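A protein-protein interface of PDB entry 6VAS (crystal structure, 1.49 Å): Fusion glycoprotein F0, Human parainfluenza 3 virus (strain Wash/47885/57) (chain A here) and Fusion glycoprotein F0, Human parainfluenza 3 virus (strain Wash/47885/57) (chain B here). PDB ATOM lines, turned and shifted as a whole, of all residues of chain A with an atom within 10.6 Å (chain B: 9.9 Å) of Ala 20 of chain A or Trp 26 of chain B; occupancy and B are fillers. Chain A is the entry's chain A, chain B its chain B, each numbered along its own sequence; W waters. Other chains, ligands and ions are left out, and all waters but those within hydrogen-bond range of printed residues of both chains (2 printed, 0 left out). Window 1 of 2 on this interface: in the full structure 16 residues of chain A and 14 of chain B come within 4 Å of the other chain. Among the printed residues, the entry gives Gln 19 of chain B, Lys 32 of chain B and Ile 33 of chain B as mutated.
Printed residues of chain B within 4 Å of Glu 12 of chain A: Ile 33 (3.8 Å). Ile 14 of chain A touches none of the printed residues of chain B. Of chain B, only Trp 26 (3.5 Å), Arg 29 (3.6 Å), Ser 30 (3.9 Å) and Ile 33 (3.4 Å) come within 4 Å of Asp 16 of chain A. Of chain B, only Ser 30 comes within 4 Å of Thr 17 of chain A. Of chain B, only Ser 23 (2.8 Å), Trp 26 (3.7 Å) and Ile 27 (3.5 Å) come within 4 Å of Ala 20 of chain A. No residue of chain B comes within 4 Å of Val 21 of chain A. Glu 21 of chain B touches none of the printed residues of chain A. Ser 23 of chain B touches three residues of chain A. Of the printed residues of chain A, Trp 26 of chain B touches Asp 16, Lys 19 and Ala 20. Ile 27 of chain B touches just one residue of chain A: Ala 20 (3.5 Å). Printed residues of chain A within 4 Å of Arg 29 of chain B: Asp 16 (3.6 Å). Ser 30 of chain B touches just these residues of chain A: Ala 13 (3.0 Å), Asp 16 (3.9 Å) and Thr 17 (3.0 Å). The nearest residue of chain A that does not touch Trp 26 of chain B is Ser 23 of chain A (4.1 Å). The nearest printed residue of chain A that does not touch Arg 29 of chain B is Ala 13 of chain A (5.9 Å).
Water W1 lies within hydrogen-bond range of the side-chain carboxylate (OE1) of Glu 22 of chain B (2.6 Å) and the side-chain hydroxyl (OG) of Ser 23 of chain A (2.7 Å). Water W2 lies within hydrogen-bond range of the indole nitrogen of Trp 26 of chain B, the side-chain carboxylate of Glu 22 of chain B and the side-chain hydroxyl of Ser 23 of chain A.
Among the printed residues, pairs that only touch across the chains: Lys 9 of chain A with Ile 33 of chain B, Ser 26 of chain A with Gln 19 of chain B, Asp 16 of chain A with Ile 33 of chain B, Val 24 of chain A with Ser 23 of chain B, Asp 16 of chain A with Trp 26 of chain B, Lys 19 of chain A with Trp 26 of chain B, Ala 20 of chain A with Ile 27 of chain B, Ser 23 of chain A with Gln 19 of chain B, Ser 23 of chain A with Ser 23 of chain B, Asp 16 of chain A with Arg 29 of chain B, Ala 20 of chain A with Trp 26 of chain B, Ala 13 of chain A with Leu 34 of chain B, Glu 12 of chain A with Ile 33 of chain B, Ser 27 of chain A with Leu 20 of chain B, Asp 16 of chain A with Ser 30 of chain B and Ala 13 of chain A with Ile 33 of chain B.
The side-chain hydroxyl of Thr 17 of chain A lies within hydrogen-bond range of the backbone carbonyl oxygen of Ala 13 of chain A, at 3.0 Å. The side-chain hydroxyl (OG) of Ser 23 of chain A lies within hydrogen-bond range of the backbone carbonyl oxygen (O) of Lys 19 of chain A. The side-chain hydroxyl (OG) of Ser 26 of chain A is in hydrogen-bond range of the backbone carbonyl oxygen (O) of Gln 22 of chain A, at 3.2 Å. The backbone carbonyl oxygen of Ser 23 of chain A is in hydrogen-bond range of the side-chain hydroxyl of Ser 27 of chain A (3.2 Å).
The backbone carbonyl oxygen (O) of Ala 13 of chain A sits at hydrogen-bond distance from the side-chain hydroxyl (OG) of Ser 30 of chain B (3.0 Å). OG1 of Thr 17 of chain A is in hydrogen-bond range of OG of Ser 30 of chain B, 3.0 Å away. The backbone carbonyl oxygen (O) of Ala 20 of chain A is in hydrogen-bond range of the side-chain hydroxyl (OG) of Ser 23 of chain B (2.8 Å). N of Ser 27 of chain A sits close to OE1 of Gln 19 of chain B (3.5 Å).
Hydrophobic or aromatic side chains of chain B within 4 Å of the printed part of chain A: Trp 26, Ile 27, Ile 33 and Leu 34.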
ATOM      1  N   LYS A   9     -31.177   7.818 -34.158  1.00  0.00           N
ATOM      2  CA  LYS A   9     -30.424   6.744 -33.518  1.00  0.00           C
ATOM      3  C   LYS A   9     -28.938   6.866 -33.827  1.00  0.00           C
ATOM      4  O   LYS A   9     -28.093   6.736 -32.935  1.00  0.00           O
ATOM      5  CB  LYS A   9     -30.963   5.388 -33.971  1.00  0.00           C
ATOM      6  CG  LYS A   9     -32.228   4.952 -33.248  1.00  0.00           C
ATOM      7  CD  LYS A   9     -32.839   3.719 -33.896  1.00  0.00           C
ATOM      8  CE  LYS A   9     -33.954   3.139 -33.039  1.00  0.00           C
ATOM      9  NZ  LYS A   9     -34.703   2.065 -33.749  1.00  0.00           N
ATOM     10  N   LYS A  11     -27.338   9.564 -34.544  1.00  0.00           N
ATOM     11  CA  LYS A  11     -26.841  10.715 -33.801  1.00  0.00           C
ATOM     12  C   LYS A  11     -26.521  10.337 -32.362  1.00  0.00           C
ATOM     13  O   LYS A  11     -25.460  10.690 -31.835  1.00  0.00           O
ATOM     14  CB  LYS A  11     -27.862  11.855 -33.840  1.00  0.00           C
ATOM     15  CG  LYS A  11     -27.558  12.967 -32.842  1.00  0.00           C
ATOM     16  CD  LYS A  11     -28.489  14.160 -33.004  1.00  0.00           C
ATOM     17  CE  LYS A  11     -28.252  15.177 -31.893  1.00  0.00           C
ATOM     18  NZ  LYS A  11     -29.141  16.368 -32.013  1.00  0.00           N
ATOM     19  N   GLU A  12     -27.438   9.630 -31.698  1.00  0.00           N
ATOM     20  CA  GLU A  12     -27.211   9.268 -30.303  1.00  0.00           C
ATOM     21  C   GLU A  12     -26.080   8.255 -30.166  1.00  0.00           C
ATOM     22  O   GLU A  12     -25.340   8.285 -29.175  1.00  0.00           O
ATOM     23  CB  GLU A  12     -28.492   8.716 -29.689  1.00  0.00           C
ATOM     24  CG  GLU A  12     -28.664   9.080 -28.222  1.00  0.00           C
ATOM     25  CD  GLU A  12     -29.607   8.147 -27.494  1.00  0.00           C
ATOM     26  OE1 GLU A  12     -29.311   7.797 -26.332  1.00  0.00           O
ATOM     27  OE2 GLU A  12     -30.637   7.757 -28.084  1.00  0.00           O
ATOM     28  N   ALA A  13     -25.930   7.354 -31.139  1.00  0.00           N
ATOM     29  CA  ALA A  13     -24.820   6.405 -31.093  1.00  0.00           C
ATOM     30  C   ALA A  13     -23.481   7.124 -31.184  1.00  0.00           C
ATOM     31  O   ALA A  13     -22.543   6.798 -30.444  1.00  0.00           O
ATOM     32  CB  ALA A  13     -24.961   5.382 -32.219  1.00  0.00           C
ATOM     33  N   ILE A  14     -23.371   8.105 -32.081  1.00  0.00           N
ATOM     34  CA  ILE A  14     -22.132   8.868 -32.191  1.00  0.00           C
ATOM     35  C   ILE A  14     -21.897   9.681 -30.929  1.00  0.00           C
ATOM     36  O   ILE A  14     -20.756   9.838 -30.482  1.00  0.00           O
ATOM     37  CB  ILE A  14     -22.156   9.765 -33.440  1.00  0.00           C
ATOM     38  CG1 ILE A  14     -22.343   8.929 -34.704  1.00  0.00           C
ATOM     39  CG2 ILE A  14     -20.865  10.576 -33.537  1.00  0.00           C
ATOM     40  CD1 ILE A  14     -22.789   9.742 -35.896  1.00  0.00           C
ATOM     41  N   ARG A  15     -22.967  10.223 -30.339  1.00  0.00           N
ATOM     42  CA  ARG A  15     -22.825  10.948 -29.084  1.00  0.00           C
ATOM     43  C   ARG A  15     -22.221  10.057 -28.011  1.00  0.00           C
ATOM     44  O   ARG A  15     -21.325  10.483 -27.269  1.00  0.00           O
ATOM     45  CB  ARG A  15     -24.182  11.475 -28.632  1.00  0.00           C
ATOM     46  CG  ARG A  15     -24.094  12.479 -27.496  1.00  0.00           C
ATOM     47  CD  ARG A  15     -23.672  13.851 -28.004  1.00  0.00           C
ATOM     48  NE  ARG A  15     -24.795  14.581 -28.590  1.00  0.00           N
ATOM     49  CZ  ARG A  15     -24.688  15.756 -29.204  1.00  0.00           C
ATOM     50  NH1 ARG A  15     -23.505  16.339 -29.328  1.00  0.00           N
ATOM     51  NH2 ARG A  15     -25.768  16.344 -29.699  1.00  0.00           N
ATOM     52  N   ASP A  16     -22.681   8.805 -27.925  1.00  0.00           N
ATOM     53  CA  ASP A  16     -22.148   7.886 -26.923  1.00  0.00           C
ATOM     54  C   ASP A  16     -20.713   7.481 -27.241  1.00  0.00           C
ATOM     55  O   ASP A  16     -19.881   7.358 -26.332  1.00  0.00           O
ATOM     56  CB  ASP A  16     -23.048   6.654 -26.817  1.00  0.00           C
ATOM     57  CG  ASP A  16     -24.409   6.976 -26.234  1.00  0.00           C
ATOM     58  OD1 ASP A  16     -24.613   8.123 -25.786  1.00  0.00           O
ATOM     59  OD2 ASP A  16     -25.278   6.078 -26.225  1.00  0.00           O
ATOM     60  N   THR A  17     -20.395   7.272 -28.523  1.00  0.00           N
ATOM     61  CA  THR A  17     -19.011   7.009 -28.898  1.00  0.00           C
ATOM     62  C   THR A  17     -18.122   8.178 -28.497  1.00  0.00           C
ATOM     63  O   THR A  17     -17.017   7.979 -27.970  1.00  0.00           O
ATOM     64  CB  THR A  17     -18.915   6.748 -30.402  1.00  0.00           C
ATOM     65  OG1 THR A  17     -19.762   5.647 -30.765  1.00  0.00           O
ATOM     66  CG2 THR A  17     -17.478   6.418 -30.798  1.00  0.00           C
ATOM     67  N   ASN A  18     -18.596   9.408 -28.716  1.00  0.00           N
ATOM     68  CA  ASN A  18     -17.817  10.584 -28.333  1.00  0.00           C
ATOM     69  C   ASN A  18     -17.584  10.618 -26.828  1.00  0.00           C
ATOM     70  O   ASN A  18     -16.483  10.947 -26.373  1.00  0.00           O
ATOM     71  CB  ASN A  18     -18.514  11.858 -28.815  1.00  0.00           C
ATOM     72  CG  ASN A  18     -18.426  12.034 -30.319  1.00  0.00           C
ATOM     73  OD1 ASN A  18     -17.717  11.294 -31.008  1.00  0.00           O
ATOM     74  ND2 ASN A  18     -19.137  13.027 -30.839  1.00  0.00           N
ATOM     75  N   LYS A  19     -18.602  10.277 -26.041  1.00  0.00           N
ATOM     76  CA  LYS A  19     -18.412  10.218 -24.594  1.00  0.00           C
ATOM     77  C   LYS A  19     -17.389   9.148 -24.215  1.00  0.00           C
ATOM     78  O   LYS A  19     -16.593   9.330 -23.285  1.00  0.00           O
ATOM     79  CB  LYS A  19     -19.759   9.995 -23.902  1.00  0.00           C
ATOM     80  CG  LYS A  19     -20.678  11.209 -23.990  1.00  0.00           C
ATOM     81  CD  LYS A  19     -22.085  10.895 -23.512  1.00  0.00           C
ATOM     82  CE  LYS A  19     -22.973  12.136 -23.556  1.00  0.00           C
ATOM     83  NZ  LYS A  19     -24.424  11.792 -23.630  1.00  0.00           N
ATOM     84  N   ALA A  20     -17.376   8.022 -24.938  1.00  0.00           N
ATOM     85  CA  ALA A  20     -16.362   7.002 -24.683  1.00  0.00           C
ATOM     86  C   ALA A  20     -14.961   7.527 -24.978  1.00  0.00           C
ATOM     87  O   ALA A  20     -14.012   7.257 -24.228  1.00  0.00           O
ATOM     88  CB  ALA A  20     -16.639   5.756 -25.521  1.00  0.00           C
ATOM     89  N   VAL A  21     -14.811   8.280 -26.067  1.00  0.00           N
ATOM     90  CA  VAL A  21     -13.511   8.855 -26.388  1.00  0.00           C
ATOM     91  C   VAL A  21     -13.103   9.874 -25.332  1.00  0.00           C
ATOM     92  O   VAL A  21     -11.937   9.935 -24.932  1.00  0.00           O
ATOM     93  CB  VAL A  21     -13.518   9.462 -27.801  1.00  0.00           C
ATOM     94  CG1 VAL A  21     -12.179  10.155 -28.087  1.00  0.00           C
ATOM     95  CG2 VAL A  21     -13.773   8.378 -28.833  1.00  0.00           C
ATOM     96  N   GLN A  22     -14.051  10.684 -24.860  1.00  0.00           N
ATOM     97  CA  GLN A  22     -13.733  11.667 -23.827  1.00  0.00           C
ATOM     98  C   GLN A  22     -13.240  10.990 -22.554  1.00  0.00           C
ATOM     99  O   GLN A  22     -12.314  11.484 -21.901  1.00  0.00           O
ATOM    100  CB  GLN A  22     -14.944  12.549 -23.544  1.00  0.00           C
ATOM    101  CG  GLN A  22     -15.264  13.507 -24.677  1.00  0.00           C
ATOM    102  CD  GLN A  22     -16.452  14.391 -24.376  1.00  0.00           C
ATOM    103  OE1 GLN A  22     -17.507  13.913 -23.958  1.00  0.00           O
ATOM    104  NE2 GLN A  22     -16.288  15.693 -24.589  1.00  0.00           N
ATOM    105  N   SER A  23     -13.841   9.857 -22.184  1.00  0.00           N
ATOM    106  CA  SER A  23     -13.359   9.121 -21.020  1.00  0.00           C
ATOM    107  C   SER A  23     -11.943   8.606 -21.251  1.00  0.00           C
ATOM    108  O   SER A  23     -11.101   8.643 -20.344  1.00  0.00           O
ATOM    109  CB  SER A  23     -14.302   7.960 -20.704  1.00  0.00           C
ATOM    110  OG  SER A  23     -15.549   8.434 -20.227  1.00  0.00           O
ATOM    111  N   VAL A  24     -11.659   8.121 -22.462  1.00  0.00           N
ATOM    112  CA  VAL A  24     -10.307   7.678 -22.794  1.00  0.00           C
ATOM    113  C   VAL A  24      -9.334   8.847 -22.724  1.00  0.00           C
ATOM    114  O   VAL A  24      -8.196   8.699 -22.263  1.00  0.00           O
ATOM    115  CB  VAL A  24     -10.295   6.997 -24.175  1.00  0.00           C
ATOM    116  CG1 VAL A  24      -8.920   7.099 -24.815  1.00  0.00           C
ATOM    117  CG2 VAL A  24     -10.714   5.541 -24.050  1.00  0.00           C
ATOM    118  N   GLN A  25      -9.762  10.023 -23.183  1.00  0.00           N
ATOM    119  CA  GLN A  25      -8.899  11.199 -23.116  1.00  0.00           C
ATOM    120  C   GLN A  25      -8.552  11.537 -21.674  1.00  0.00           C
ATOM    121  O   GLN A  25      -7.397  11.866 -21.365  1.00  0.00           O
ATOM    122  CB  GLN A  25      -9.587  12.384 -23.790  1.00  0.00           C
ATOM    123  CG  GLN A  25      -9.705  12.264 -25.299  1.00  0.00           C
ATOM    124  CD  GLN A  25     -10.703  13.242 -25.893  1.00  0.00           C
ATOM    125  OE1 GLN A  25     -11.486  13.871 -25.176  1.00  0.00           O
ATOM    126  NE2 GLN A  25     -10.676  13.381 -27.210  1.00  0.00           N
ATOM    127  N   SER A  26      -9.538  11.473 -20.777  1.00  0.00           N
ATOM    128  CA  SER A  26      -9.264  11.727 -19.365  1.00  0.00           C
ATOM    129  C   SER A  26      -8.296  10.691 -18.807  1.00  0.00           C
ATOM    130  O   SER A  26      -7.413  11.021 -18.004  1.00  0.00           O
ATOM    131  CB  SER A  26     -10.571  11.721 -18.575  1.00  0.00           C
ATOM    132  OG  SER A  26     -11.478  12.689 -19.075  1.00  0.00           O
ATOM    133  N   SER A  27      -8.442   9.433 -19.230  1.00  0.00           N
ATOM    134  CA  SER A  27      -7.530   8.385 -18.784  1.00  0.00           C
ATOM    135  C   SER A  27      -6.101   8.672 -19.227  1.00  0.00           C
ATOM    136  O   SER A  27      -5.151   8.472 -18.458  1.00  0.00           O
ATOM    137  CB  SER A  27      -7.982   7.031 -19.334  1.00  0.00           C
ATOM    138  OG  SER A  27      -9.227   6.644 -18.786  1.00  0.00           O
ATOM    139  N   ILE A  28      -5.927   9.140 -20.464  1.00  0.00           N
ATOM    140  CA  ILE A  28      -4.584   9.411 -20.969  1.00  0.00           C
ATOM    141  C   ILE A  28      -3.941  10.555 -20.198  1.00  0.00           C
ATOM    142  O   ILE A  28      -2.738  10.525 -19.902  1.00  0.00           O
ATOM    143  CB  ILE A  28      -4.625   9.672 -22.487  1.00  0.00           C
ATOM    144  CG1 ILE A  28      -4.880   8.356 -23.226  1.00  0.00           C
ATOM    145  CG2 ILE A  28      -3.328  10.317 -22.952  1.00  0.00           C
ATOM    146  CD1 ILE A  28      -5.314   8.532 -24.658  1.00  0.00           C
ATOM    147  N   SER B  18     -11.364   3.500 -13.276  1.00  0.00           N
ATOM    148  CA  SER B  18     -12.761   3.925 -13.256  1.00  0.00           C
ATOM    149  C   SER B  18     -13.142   4.617 -14.560  1.00  0.00           C
ATOM    150  O   SER B  18     -14.211   4.349 -15.122  1.00  0.00           O
ATOM    151  CB  SER B  18     -13.007   4.851 -12.067  1.00  0.00           C
ATOM    152  OG  SER B  18     -14.374   5.201 -11.970  1.00  0.00           O
ATOM    153  N   GLN B  19     -12.284   5.512 -15.052  1.00  0.00           N
ATOM    154  CA  GLN B  19     -12.561   6.177 -16.320  1.00  0.00           C
ATOM    155  C   GLN B  19     -12.597   5.184 -17.474  1.00  0.00           C
ATOM    156  O   GLN B  19     -13.384   5.346 -18.412  1.00  0.00           O
ATOM    157  CB  GLN B  19     -11.511   7.261 -16.568  1.00  0.00           C
ATOM    158  CG  GLN B  19     -11.543   8.378 -15.545  1.00  0.00           C
ATOM    159  CD  GLN B  19     -10.354   9.309 -15.652  1.00  0.00           C
ATOM    160  OE1 GLN B  19      -9.226   8.872 -15.888  1.00  0.00           O
ATOM    161  NE2 GLN B  19     -10.598  10.602 -15.476  1.00  0.00           N
ATOM    162  N   LEU B  20     -11.759   4.146 -17.420  1.00  0.00           N
ATOM    163  CA  LEU B  20     -11.800   3.111 -18.447  1.00  0.00           C
ATOM    164  C   LEU B  20     -13.114   2.341 -18.399  1.00  0.00           C
ATOM    165  O   LEU B  20     -13.691   2.022 -19.447  1.00  0.00           O
ATOM    166  CB  LEU B  20     -10.610   2.169 -18.267  1.00  0.00           C
ATOM    167  CG  LEU B  20     -10.274   1.212 -19.408  1.00  0.00           C
ATOM    168  CD1 LEU B  20      -9.969   1.972 -20.687  1.00  0.00           C
ATOM    169  CD2 LEU B  20      -9.098   0.325 -19.012  1.00  0.00           C
ATOM    170  N   GLU B  21     -13.610   2.045 -17.194  1.00  0.00           N
ATOM    171  CA  GLU B  21     -14.896   1.369 -17.066  1.00  0.00           C
ATOM    172  C   GLU B  21     -16.021   2.202 -17.669  1.00  0.00           C
ATOM    173  O   GLU B  21     -16.892   1.666 -18.370  1.00  0.00           O
ATOM    174  CB  GLU B  21     -15.192   1.086 -15.592  1.00  0.00           C
ATOM    175  CG  GLU B  21     -14.308   0.024 -14.969  1.00  0.00           C
ATOM    176  CD  GLU B  21     -14.998  -0.708 -13.836  1.00  0.00           C
ATOM    177  OE1 GLU B  21     -15.380  -0.050 -12.844  1.00  0.00           O
ATOM    178  OE2 GLU B  21     -15.173  -1.939 -13.948  1.00  0.00           O
ATOM    179  N   GLU B  22     -16.030   3.508 -17.398  1.00  0.00           N
ATOM    180  CA  GLU B  22     -17.048   4.376 -17.977  1.00  0.00           C
ATOM    181  C   GLU B  22     -16.983   4.358 -19.499  1.00  0.00           C
ATOM    182  O   GLU B  22     -18.020   4.287 -20.177  1.00  0.00           O
ATOM    183  CB  GLU B  22     -16.870   5.801 -17.451  1.00  0.00           C
ATOM    184  CG  GLU B  22     -17.021   5.927 -15.944  1.00  0.00           C
ATOM    185  CD  GLU B  22     -16.773   7.336 -15.444  1.00  0.00           C
ATOM    186  OE1 GLU B  22     -16.604   8.248 -16.283  1.00  0.00           O
ATOM    187  OE2 GLU B  22     -16.758   7.533 -14.210  1.00  0.00           O
ATOM    188  N   SER B  23     -15.772   4.420 -20.056  1.00  0.00           N
ATOM    189  CA  SER B  23     -15.620   4.414 -21.505  1.00  0.00           C
ATOM    190  C   SER B  23     -16.204   3.147 -22.112  1.00  0.00           C
ATOM    191  O   SER B  23     -16.906   3.205 -23.131  1.00  0.00           O
ATOM    192  CB  SER B  23     -14.141   4.544 -21.864  1.00  0.00           C
ATOM    193  OG  SER B  23     -13.957   4.665 -23.263  1.00  0.00           O
ATOM    194  N   LYS B  24     -15.928   1.994 -21.504  1.00  0.00           N
ATOM    195  CA  LYS B  24     -16.452   0.737 -22.025  1.00  0.00           C
ATOM    196  C   LYS B  24     -17.975   0.721 -21.988  1.00  0.00           C
ATOM    197  O   LYS B  24     -18.624   0.184 -22.891  1.00  0.00           O
ATOM    198  CB  LYS B  24     -15.869  -0.433 -21.234  1.00  0.00           C
ATOM    199  CG  LYS B  24     -14.376  -0.623 -21.456  1.00  0.00           C
ATOM    200  CD  LYS B  24     -13.801  -1.735 -20.591  1.00  0.00           C
ATOM    201  CE  LYS B  24     -12.316  -1.924 -20.875  1.00  0.00           C
ATOM    202  NZ  LYS B  24     -11.647  -2.780 -19.855  1.00  0.00           N
ATOM    203  N   GLU B  25     -18.573   1.324 -20.958  1.00  0.00           N
ATOM    204  CA  GLU B  25     -20.031   1.351 -20.875  1.00  0.00           C
ATOM    205  C   GLU B  25     -20.635   2.242 -21.958  1.00  0.00           C
ATOM    206  O   GLU B  25     -21.689   1.915 -22.520  1.00  0.00           O
ATOM    207  CB  GLU B  25     -20.466   1.804 -19.480  1.00  0.00           C
ATOM    208  CG  GLU B  25     -21.937   1.576 -19.168  1.00  0.00           C
ATOM    209  CD  GLU B  25     -22.377   0.145 -19.418  1.00  0.00           C
ATOM    210  OE1 GLU B  25     -23.374  -0.052 -20.145  1.00  0.00           O
ATOM    211  OE2 GLU B  25     -21.718  -0.780 -18.904  1.00  0.00           O
ATOM    212  N   TRP B  26     -19.980   3.363 -22.277  1.00  0.00           N
ATOM    213  CA  TRP B  26     -20.493   4.230 -23.337  1.00  0.00           C
ATOM    214  C   TRP B  26     -20.463   3.524 -24.690  1.00  0.00           C
ATOM    215  O   TRP B  26     -21.351   3.728 -25.524  1.00  0.00           O
ATOM    216  CB  TRP B  26     -19.688   5.531 -23.399  1.00  0.00           C
ATOM    217  CG  TRP B  26     -20.040   6.525 -22.341  1.00  0.00           C
ATOM    218  CD1 TRP B  26     -19.218   7.015 -21.366  1.00  0.00           C
ATOM    219  CD2 TRP B  26     -21.313   7.148 -22.141  1.00  0.00           C
ATOM    220  NE1 TRP B  26     -19.900   7.908 -20.578  1.00  0.00           N
ATOM    221  CE2 TRP B  26     -21.188   8.008 -21.033  1.00  0.00           C
ATOM    222  CE3 TRP B  26     -22.547   7.063 -22.795  1.00  0.00           C
ATOM    223  CZ2 TRP B  26     -22.248   8.770 -20.558  1.00  0.00           C
ATOM    224  CZ3 TRP B  26     -23.597   7.826 -22.326  1.00  0.00           C
ATOM    225  CH2 TRP B  26     -23.443   8.671 -21.219  1.00  0.00           C
ATOM    226  N   ILE B  27     -19.443   2.699 -24.933  1.00  0.00           N
ATOM    227  CA  ILE B  27     -19.389   1.942 -26.182  1.00  0.00           C
ATOM    228  C   ILE B  27     -20.482   0.879 -26.209  1.00  0.00           C
ATOM    229  O   ILE B  27     -21.109   0.642 -27.250  1.00  0.00           O
ATOM    230  CB  ILE B  27     -17.989   1.336 -26.390  1.00  0.00           C
ATOM    231  CG1 ILE B  27     -16.969   2.437 -26.687  1.00  0.00           C
ATOM    232  CG2 ILE B  27     -18.021   0.297 -27.514  1.00  0.00           C
ATOM    233  CD1 ILE B  27     -17.194   3.165 -28.005  1.00  0.00           C
ATOM    234  N   ARG B  28     -20.725   0.218 -25.071  1.00  0.00           N
ATOM    235  CA  ARG B  28     -21.815  -0.754 -25.005  1.00  0.00           C
ATOM    236  C   ARG B  28     -23.141  -0.104 -25.375  1.00  0.00           C
ATOM    237  O   ARG B  28     -23.946  -0.687 -26.114  1.00  0.00           O
ATOM    238  CB  ARG B  28     -21.896  -1.374 -23.609  1.00  0.00           C
ATOM    239  CG  ARG B  28     -20.710  -2.256 -23.240  1.00  0.00           C
ATOM    240  CD  ARG B  28     -20.932  -2.974 -21.906  1.00  0.00           C
ATOM    241  NE  ARG B  28     -19.698  -3.555 -21.377  1.00  0.00           N
ATOM    242  CZ  ARG B  28     -19.018  -3.072 -20.338  1.00  0.00           C
ATOM    243  NH1 ARG B  28     -19.442  -1.996 -19.688  1.00  0.00           N
ATOM    244  NH2 ARG B  28     -17.905  -3.676 -19.941  1.00  0.00           N
ATOM    245  N   ARG B  29     -23.386   1.111 -24.876  1.00  0.00           N
ATOM    246  CA  ARG B  29     -24.633   1.798 -25.196  1.00  0.00           C
ATOM    247  C   ARG B  29     -24.693   2.169 -26.674  1.00  0.00           C
ATOM    248  O   ARG B  29     -25.733   1.997 -27.320  1.00  0.00           O
ATOM    249  CB  ARG B  29     -24.788   3.041 -24.320  1.00  0.00           C
ATOM    250  CG  ARG B  29     -25.041   2.727 -22.856  1.00  0.00           C
ATOM    251  CD  ARG B  29     -25.597   3.932 -22.111  1.00  0.00           C
ATOM    252  NE  ARG B  29     -26.185   3.550 -20.829  1.00  0.00           N
ATOM    253  CZ  ARG B  29     -27.453   3.179 -20.663  1.00  0.00           C
ATOM    254  NH1 ARG B  29     -28.281   3.136 -21.699  1.00  0.00           N
ATOM    255  NH2 ARG B  29     -27.892   2.848 -19.457  1.00  0.00           N
ATOM    256  N   SER B  30     -23.594   2.680 -27.226  1.00  0.00           N
ATOM    257  CA  SER B  30     -23.562   3.004 -28.648  1.00  0.00           C
ATOM    258  C   SER B  30     -23.880   1.776 -29.493  1.00  0.00           C
ATOM    259  O   SER B  30     -24.680   1.842 -30.433  1.00  0.00           O
ATOM    260  CB  SER B  30     -22.197   3.585 -29.024  1.00  0.00           C
ATOM    261  OG  SER B  30     -22.118   3.833 -30.419  1.00  0.00           O
ATOM    262  N   ASN B  31     -23.258   0.636 -29.170  1.00  0.00           N
ATOM    263  CA  ASN B  31     -23.487  -0.578 -29.950  1.00  0.00           C
ATOM    264  C   ASN B  31     -24.928  -1.066 -29.830  1.00  0.00           C
ATOM    265  O   ASN B  31     -25.512  -1.527 -30.819  1.00  0.00           O
ATOM    266  CB  ASN B  31     -22.506  -1.671 -29.524  1.00  0.00           C
ATOM    267  CG  ASN B  31     -21.127  -1.478 -30.115  1.00  0.00           C
ATOM    268  OD1 ASN B  31     -20.980  -0.917 -31.200  1.00  0.00           O
ATOM    269  ND2 ASN B  31     -20.108  -1.947 -29.407  1.00  0.00           N
ATOM    270  N   LYS B  32     -25.522  -0.970 -28.638  1.00  0.00           N
ATOM    271  CA  LYS B  32     -26.922  -1.361 -28.490  1.00  0.00           C
ATOM    272  C   LYS B  32     -27.828  -0.488 -29.349  1.00  0.00           C
ATOM    273  O   LYS B  32     -28.783  -0.981 -29.962  1.00  0.00           O
ATOM    274  CB  LYS B  32     -27.343  -1.275 -27.024  1.00  0.00           C
ATOM    275  CG  LYS B  32     -26.781  -2.378 -26.141  1.00  0.00           C
ATOM    276  CD  LYS B  32     -27.287  -2.238 -24.712  1.00  0.00           C
ATOM    277  CE  LYS B  32     -26.404  -2.985 -23.725  1.00  0.00           C
ATOM    278  NZ  LYS B  32     -26.356  -2.279 -22.410  1.00  0.00           N
ATOM    279  N   ILE B  33     -27.549   0.816 -29.400  1.00  0.00           N
ATOM    280  CA  ILE B  33     -28.312   1.703 -30.271  1.00  0.00           C
ATOM    281  C   ILE B  33     -28.167   1.269 -31.724  1.00  0.00           C
ATOM    282  O   ILE B  33     -29.147   1.206 -32.474  1.00  0.00           O
ATOM    283  CB  ILE B  33     -27.878   3.167 -30.066  1.00  0.00           C
ATOM    284  CG1 ILE B  33     -28.273   3.642 -28.664  1.00  0.00           C
ATOM    285  CG2 ILE B  33     -28.499   4.049 -31.138  1.00  0.00           C
ATOM    286  CD1 ILE B  33     -27.693   4.992 -28.285  1.00  0.00           C
ATOM    287  N   LEU B  34     -26.937   0.963 -32.143  1.00  0.00           N
ATOM    288  CA  LEU B  34     -26.716   0.525 -33.516  1.00  0.00           C
ATOM    289  C   LEU B  34     -27.493  -0.750 -33.823  1.00  0.00           C
ATOM    290  O   LEU B  34     -28.022  -0.912 -34.929  1.00  0.00           O
ATOM    291  CB  LEU B  34     -25.223   0.312 -33.764  1.00  0.00           C
ATOM    292  CG  LEU B  34     -24.329   1.552 -33.717  1.00  0.00           C
ATOM    293  CD1 LEU B  34     -22.879   1.124 -33.950  1.00  0.00           C
ATOM    294  CD2 LEU B  34     -24.752   2.590 -34.735  1.00  0.00           C
HETATM  295  O   HOH W   1     -14.579   8.790 -17.752  1.00  0.00           O
HETATM  296  O   HOH W   2     -18.307   9.540 -18.698  1.00  0.00           O
